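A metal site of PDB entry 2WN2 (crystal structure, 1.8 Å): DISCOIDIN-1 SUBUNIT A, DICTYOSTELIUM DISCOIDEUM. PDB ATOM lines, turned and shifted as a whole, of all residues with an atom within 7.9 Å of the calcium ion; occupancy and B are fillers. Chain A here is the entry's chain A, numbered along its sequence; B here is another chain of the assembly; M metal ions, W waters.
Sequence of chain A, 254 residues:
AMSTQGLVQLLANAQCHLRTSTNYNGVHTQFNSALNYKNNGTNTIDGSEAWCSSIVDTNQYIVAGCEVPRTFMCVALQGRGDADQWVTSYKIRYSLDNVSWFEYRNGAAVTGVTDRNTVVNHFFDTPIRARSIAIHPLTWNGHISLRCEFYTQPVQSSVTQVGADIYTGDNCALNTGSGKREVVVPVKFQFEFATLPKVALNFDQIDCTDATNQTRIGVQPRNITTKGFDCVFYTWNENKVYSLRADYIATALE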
ATOM      1  N   GLY A 163      -1.559 -21.183 -15.636  1.00  0.00           N
ATOM      2  CA  GLY A 163      -0.447 -20.273 -15.698  1.00  0.00           C
ATOM      3  C   GLY A 163       0.823 -21.059 -15.709  1.00  0.00           C
ATOM      4  O   GLY A 163       0.960 -22.063 -14.998  1.00  0.00           O
ATOM      5  N   ALA A 164       1.794 -20.589 -16.496  1.00  0.00           N
ATOM      6  CA  ALA A 164       2.955 -21.379 -16.796  1.00  0.00           C
ATOM      7  C   ALA A 164       4.171 -20.744 -16.161  1.00  0.00           C
ATOM      8  O   ALA A 164       4.294 -19.526 -16.065  1.00  0.00           O
ATOM      9  CB  ALA A 164       3.174 -21.466 -18.297  1.00  0.00           C
ATOM     10  N   ASP A 165       5.111 -21.630 -15.834  1.00  0.00           N
ATOM     11  CA  ASP A 165       6.519 -21.247 -15.615  1.00  0.00           C
ATOM     12  C   ASP A 165       6.800 -20.300 -14.449  1.00  0.00           C
ATOM     13  O   ASP A 165       7.619 -19.395 -14.565  1.00  0.00           O
ATOM     14  CB  ASP A 165       7.075 -20.658 -16.903  1.00  0.00           C
ATOM     15  CG  ASP A 165       6.835 -21.560 -18.104  1.00  0.00           C
ATOM     16  OD1 ASP A 165       6.722 -22.765 -17.893  1.00  0.00           O
ATOM     17  OD2 ASP A 165       6.809 -21.052 -19.234  1.00  0.00           O
ATOM     18  N   ILE A 166       6.187 -20.585 -13.294  1.00  0.00           N
ATOM     19  CA  ILE A 166       6.482 -19.813 -12.085  1.00  0.00           C
ATOM     20  C   ILE A 166       7.886 -20.313 -11.647  1.00  0.00           C
ATOM     21  O   ILE A 166       8.097 -21.491 -11.625  1.00  0.00           O
ATOM     22  CB  ILE A 166       5.485 -20.131 -10.985  1.00  0.00           C
ATOM     23  CG1 ILE A 166       4.033 -20.030 -11.511  1.00  0.00           C
ATOM     24  CG2 ILE A 166       5.719 -19.178  -9.799  1.00  0.00           C
ATOM     25  CD1 ILE A 166       3.753 -18.688 -12.213  1.00  0.00           C
ATOM     26  N   ASN A 202       2.548 -28.000  -9.979  1.00  0.00           N
ATOM     27  CA  ASN A 202       3.389 -29.170 -10.147  1.00  0.00           C
ATOM     28  C   ASN A 202       4.661 -28.836 -10.934  1.00  0.00           C
ATOM     29  O   ASN A 202       4.699 -27.858 -11.684  1.00  0.00           O
ATOM     30  CB  ASN A 202       2.572 -30.238 -10.900  1.00  0.00           C
ATOM     31  CG  ASN A 202       1.337 -30.655 -10.155  1.00  0.00           C
ATOM     32  OD1 ASN A 202       0.221 -30.506 -10.672  1.00  0.00           O
ATOM     33  ND2 ASN A 202       1.510 -31.127  -8.917  1.00  0.00           N
ATOM     34  N   PHE A 203       5.698 -29.679 -10.769  1.00  0.00           N
ATOM     35  CA  PHE A 203       7.026 -29.360 -11.316  1.00  0.00           C
ATOM     36  C   PHE A 203       7.118 -29.510 -12.827  1.00  0.00           C
ATOM     37  O   PHE A 203       6.604 -30.478 -13.380  1.00  0.00           O
ATOM     38  CB  PHE A 203       8.118 -30.283 -10.732  1.00  0.00           C
ATOM     39  CG  PHE A 203       8.317 -30.145  -9.248  1.00  0.00           C
ATOM     40  CD1 PHE A 203       8.035 -31.210  -8.380  1.00  0.00           C
ATOM     41  CD2 PHE A 203       8.815 -28.974  -8.713  1.00  0.00           C
ATOM     42  CE1 PHE A 203       8.222 -31.080  -7.044  1.00  0.00           C
ATOM     43  CE2 PHE A 203       9.027 -28.821  -7.337  1.00  0.00           C
ATOM     44  CZ  PHE A 203       8.747 -29.874  -6.504  1.00  0.00           C
ATOM     45  N   ASP A 204       7.813 -28.591 -13.464  1.00  0.00           N
ATOM     46  CA  ASP A 204       8.248 -28.795 -14.840  1.00  0.00           C
ATOM     47  C   ASP A 204       9.773 -28.660 -15.067  1.00  0.00           C
ATOM     48  O   ASP A 204      10.255 -28.974 -16.167  1.00  0.00           O
ATOM     49  CB  ASP A 204       7.489 -27.920 -15.846  1.00  0.00           C
ATOM     50  CG  ASP A 204       7.795 -26.463 -15.692  1.00  0.00           C
ATOM     51  OD1 ASP A 204       8.256 -26.083 -14.611  1.00  0.00           O
ATOM     52  OD2 ASP A 204       7.633 -25.665 -16.690  1.00  0.00           O
ATOM     53  N   GLN A 205      10.522 -28.147 -14.076  1.00  0.00           N
ATOM     54  CA  GLN A 205      11.990 -28.102 -14.204  1.00  0.00           C
ATOM     55  C   GLN A 205      12.623 -28.183 -12.836  1.00  0.00           C
ATOM     56  O   GLN A 205      12.244 -27.454 -11.938  1.00  0.00           O
ATOM     57  CB  GLN A 205      12.439 -26.834 -14.911  1.00  0.00           C
ATOM     58  CG  GLN A 205      13.894 -26.823 -15.352  1.00  0.00           C
ATOM     59  CD  GLN A 205      14.320 -25.514 -15.949  1.00  0.00           C
ATOM     60  OE1 GLN A 205      14.451 -25.399 -17.176  1.00  0.00           O
ATOM     61  NE2 GLN A 205      14.587 -24.520 -15.108  1.00  0.00           N
ATOM     62  N   ARG A 245      10.922 -24.957 -11.075  1.00  0.00           N
ATOM     63  CA  ARG A 245       9.895 -24.297 -11.857  1.00  0.00           C
ATOM     64  C   ARG A 245       8.633 -25.155 -11.790  1.00  0.00           C
ATOM     65  O   ARG A 245       8.687 -26.395 -11.669  1.00  0.00           O
ATOM     66  CB  ARG A 245      10.367 -24.071 -13.304  1.00  0.00           C
ATOM     67  CG  ARG A 245       9.674 -22.957 -14.065  1.00  0.00           C
ATOM     68  CD  ARG A 245      10.247 -22.777 -15.456  1.00  0.00           C
ATOM     69  NE  ARG A 245       9.977 -23.973 -16.250  1.00  0.00           N
ATOM     70  CZ  ARG A 245      10.656 -24.341 -17.301  1.00  0.00           C
ATOM     71  NH1 ARG A 245      11.669 -23.619 -17.714  1.00  0.00           N
ATOM     72  NH2 ARG A 245      10.271 -25.439 -17.990  1.00  0.00           N
ATOM     73  N   ALA A 246       7.505 -24.478 -11.908  1.00  0.00           N
ATOM     74  CA  ALA A 246       6.215 -25.154 -11.868  1.00  0.00           C
ATOM     75  C   ALA A 246       5.196 -24.474 -12.738  1.00  0.00           C
ATOM     76  O   ALA A 246       5.283 -23.281 -12.942  1.00  0.00           O
ATOM     77  CB  ALA A 246       5.692 -25.165 -10.418  1.00  0.00           C
ATOM     78  N   ASP A 247       4.220 -25.226 -13.223  1.00  0.00           N
ATOM     79  CA  ASP A 247       3.010 -24.670 -13.888  1.00  0.00           C
ATOM     80  C   ASP A 247       1.822 -24.884 -12.935  1.00  0.00           C
ATOM     81  O   ASP A 247       1.875 -25.790 -12.080  1.00  0.00           O
ATOM     82  CB  ASP A 247       2.729 -25.348 -15.227  1.00  0.00           C
ATOM     83  CG  ASP A 247       3.871 -25.245 -16.211  1.00  0.00           C
ATOM     84  OD1 ASP A 247       4.597 -24.270 -16.176  1.00  0.00           O
ATOM     85  OD2 ASP A 247       4.024 -26.199 -16.969  1.00  0.00           O
ATOM     86  N   TYR A 248       0.793 -24.036 -13.015  1.00  0.00           N
ATOM     87  CA  TYR A 248      -0.405 -24.210 -12.183  1.00  0.00           C
ATOM     88  C   TYR A 248      -1.688 -24.317 -13.006  1.00  0.00           C
ATOM     89  O   TYR A 248      -1.777 -23.839 -14.162  1.00  0.00           O
ATOM     90  CB  TYR A 248      -0.558 -23.105 -11.127  1.00  0.00           C
ATOM     91  CG  TYR A 248      -1.009 -21.773 -11.609  1.00  0.00           C
ATOM     92  CD1 TYR A 248      -0.079 -20.750 -11.914  1.00  0.00           C
ATOM     93  CD2 TYR A 248      -2.342 -21.513 -11.803  1.00  0.00           C
ATOM     94  CE1 TYR A 248      -0.513 -19.516 -12.343  1.00  0.00           C
ATOM     95  CE2 TYR A 248      -2.774 -20.271 -12.233  1.00  0.00           C
ATOM     96  CZ  TYR A 248      -1.854 -19.285 -12.530  1.00  0.00           C
ATOM     97  OH  TYR A 248      -2.306 -18.063 -12.980  1.00  0.00           O
ATOM     98  N   VAL B 199      -0.709 -23.740 -21.578  1.00  0.00           N
ATOM     99  CA  VAL B 199      -0.457 -25.185 -21.375  1.00  0.00           C
ATOM    100  C   VAL B 199       0.446 -25.382 -20.147  1.00  0.00           C
ATOM    101  O   VAL B 199       1.543 -24.809 -20.074  1.00  0.00           O
ATOM    102  CB  VAL B 199       0.175 -25.854 -22.596  1.00  0.00           C
ATOM    103  CG1 VAL B 199       0.391 -27.353 -22.343  1.00  0.00           C
ATOM    104  CG2 VAL B 199      -0.711 -25.667 -23.849  1.00  0.00           C
ATOM    105  N   ALA B 200      -0.052 -26.173 -19.215  1.00  0.00           N
ATOM    106  CA  ALA B 200       0.685 -26.727 -18.082  1.00  0.00           C
ATOM    107  C   ALA B 200       1.135 -28.118 -18.531  1.00  0.00           C
ATOM    108  O   ALA B 200       0.354 -28.865 -19.133  1.00  0.00           O
ATOM    109  CB  ALA B 200      -0.236 -26.857 -16.848  1.00  0.00           C
ATOM    110  N   LEU B 201       2.397 -28.441 -18.282  1.00  0.00           N
ATOM    111  CA  LEU B 201       2.999 -29.715 -18.730  1.00  0.00           C
ATOM    112  C   LEU B 201       4.022 -30.105 -17.697  1.00  0.00           C
ATOM    113  O   LEU B 201       5.074 -29.449 -17.551  1.00  0.00           O
ATOM    114  CB  LEU B 201       3.647 -29.485 -20.086  1.00  0.00           C
ATOM    115  CG  LEU B 201       4.429 -30.601 -20.751  1.00  0.00           C
ATOM    116  CD1 LEU B 201       3.608 -31.755 -21.182  1.00  0.00           C
ATOM    117  CD2 LEU B 201       5.214 -29.956 -21.982  1.00  0.00           C
ATOM    118  N   ASN B 202       3.673 -31.122 -16.932  1.00  0.00           N
ATOM    119  CA  ASN B 202       4.362 -31.408 -15.653  1.00  0.00           C
ATOM    120  C   ASN B 202       4.669 -32.922 -15.545  1.00  0.00           C
ATOM    121  O   ASN B 202       4.008 -33.740 -16.174  1.00  0.00           O
ATOM    122  CB  ASN B 202       3.491 -30.954 -14.499  1.00  0.00           C
ATOM    123  CG  ASN B 202       3.167 -29.470 -14.570  1.00  0.00           C
ATOM    124  OD1 ASN B 202       1.998 -29.096 -14.621  1.00  0.00           O
ATOM    125  ND2 ASN B 202       4.176 -28.650 -14.597  1.00  0.00           N
ATOM    126  N   VAL B 219      10.780 -30.073 -18.778  1.00  0.00           N
ATOM    127  CA  VAL B 219       9.796 -30.364 -19.822  1.00  0.00           C
ATOM    128  C   VAL B 219       9.049 -29.059 -20.032  1.00  0.00           C
ATOM    129  O   VAL B 219       8.756 -28.352 -19.076  1.00  0.00           O
ATOM    130  CB  VAL B 219       8.850 -31.538 -19.498  1.00  0.00           C
ATOM    131  CG1 VAL B 219       7.947 -31.292 -18.272  1.00  0.00           C
ATOM    132  CG2 VAL B 219       8.026 -31.987 -20.769  1.00  0.00           C
ATOM    133  N   GLN B 220       8.772 -28.754 -21.288  1.00  0.00           N
ATOM    134  CA  GLN B 220       8.197 -27.459 -21.659  1.00  0.00           C
ATOM    135  C   GLN B 220       7.514 -27.511 -23.022  1.00  0.00           C
ATOM    136  O   GLN B 220       8.043 -28.131 -23.960  1.00  0.00           O
ATOM    137  CB  GLN B 220       9.317 -26.429 -21.700  1.00  0.00           C
ATOM    138  CG  GLN B 220       8.890 -24.990 -21.962  1.00  0.00           C
ATOM    139  CD  GLN B 220       8.179 -24.355 -20.750  1.00  0.00           C
ATOM    140  OE1 GLN B 220       7.614 -25.042 -19.915  1.00  0.00           O
ATOM    141  NE2 GLN B 220       8.283 -23.012 -20.641  1.00  0.00           N
ATOM    142  N   PRO B 221       6.351 -26.847 -23.143  1.00  0.00           N
ATOM    143  CA  PRO B 221       5.790 -26.707 -24.491  1.00  0.00           C
ATOM    144  C   PRO B 221       6.530 -25.723 -25.350  1.00  0.00           C
ATOM    145  O   PRO B 221       7.130 -24.740 -24.866  1.00  0.00           O
ATOM    146  CB  PRO B 221       4.375 -26.189 -24.245  1.00  0.00           C
ATOM    147  CG  PRO B 221       4.136 -26.310 -22.754  1.00  0.00           C
ATOM    148  CD  PRO B 221       5.468 -26.281 -22.121  1.00  0.00           C
ATOM    149  N   TYR B 234      13.960 -32.228 -21.809  1.00  0.00           N
ATOM    150  CA  TYR B 234      15.380 -31.825 -21.912  1.00  0.00           C
ATOM    151  C   TYR B 234      16.188 -32.048 -20.634  1.00  0.00           C
ATOM    152  O   TYR B 234      15.648 -32.268 -19.576  1.00  0.00           O
ATOM    153  CB  TYR B 234      15.514 -30.353 -22.333  1.00  0.00           C
ATOM    154  CG  TYR B 234      14.825 -29.350 -21.445  1.00  0.00           C
ATOM    155  CD1 TYR B 234      15.497 -28.727 -20.439  1.00  0.00           C
ATOM    156  CD2 TYR B 234      13.432 -29.092 -21.577  1.00  0.00           C
ATOM    157  CE1 TYR B 234      14.853 -27.806 -19.623  1.00  0.00           C
ATOM    158  CE2 TYR B 234      12.790 -28.201 -20.752  1.00  0.00           C
ATOM    159  CZ  TYR B 234      13.500 -27.559 -19.754  1.00  0.00           C
ATOM    160  OH  TYR B 234      12.866 -26.640 -18.935  1.00  0.00           O
HETATM  161 CA    CA M   1       5.954 -25.045 -18.118  1.00  0.00          CA
HETATM  162  O   HOH W   1       6.147 -27.369 -18.838  1.00  0.00           O
HETATM  163  O   HOH W   2       4.327 -24.448 -19.783  1.00  0.00           O
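The side-chain carboxylate of Asp 247 sits close to the backbone NH of Leu 201 of chain B, 3.1 Å away. The side-chain amide oxygen of Gln 220 of chain B sits close to the guanidinium group of Arg 245 (3.3 Å). The backbone carbonyl oxygen (O) of Asp 204 is in hydrogen-bond range of the backbone NH (N) of Val 219 of chain B, at 2.9 Å. The side-chain carboxylate of Asp 165 sits close to the guanidinium group of Arg 245 (3.8 Å). N of Ala 246 sits at hydrogen-bond distance from OD1 of Asp 204 (3.2 Å). N of Asp 247 lies within hydrogen-bond range of O of Asn 202 of chain A (3.1 Å). The backbone NH of Asp 165 sits at hydrogen-bond distance from the backbone carbonyl oxygen of Ala 246 (3.3 Å). OD1 of Asp 204 lies within salt-bridge range of NE of Arg 245.
Four residues have an atom within 4 Å of the calcium ion: Asp 165, Asp 204, Asp 247 and Gln 220 of chain B. The nearest printed residue that does not touch the calcium ion is Pro 221 of chain B (4.2 Å).
The calcium ion is bound by the side-chain carboxylate (OD2) of Asp 204. Water W2 is bound to the calcium ion. The calcium ion is bound by OD1 of Asp 165, at 2.4 Å. Water W1 is bound to the calcium ion, at 2.4 Å. The calcium ion is bound by the side-chain amide oxygen (OE1) of Gln 220 of chain B (2.4 Å). OD1 of Asp 247 is bound to the calcium ion (2.5 Å). OD2 of Asp 247 is bound to the calcium ion.
Water W1 lies within hydrogen-bond range of the backbone carbonyl oxygen (O) of Leu 201 of chain B and the backbone carbonyl oxygen (O) of Val 219 of chain B.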
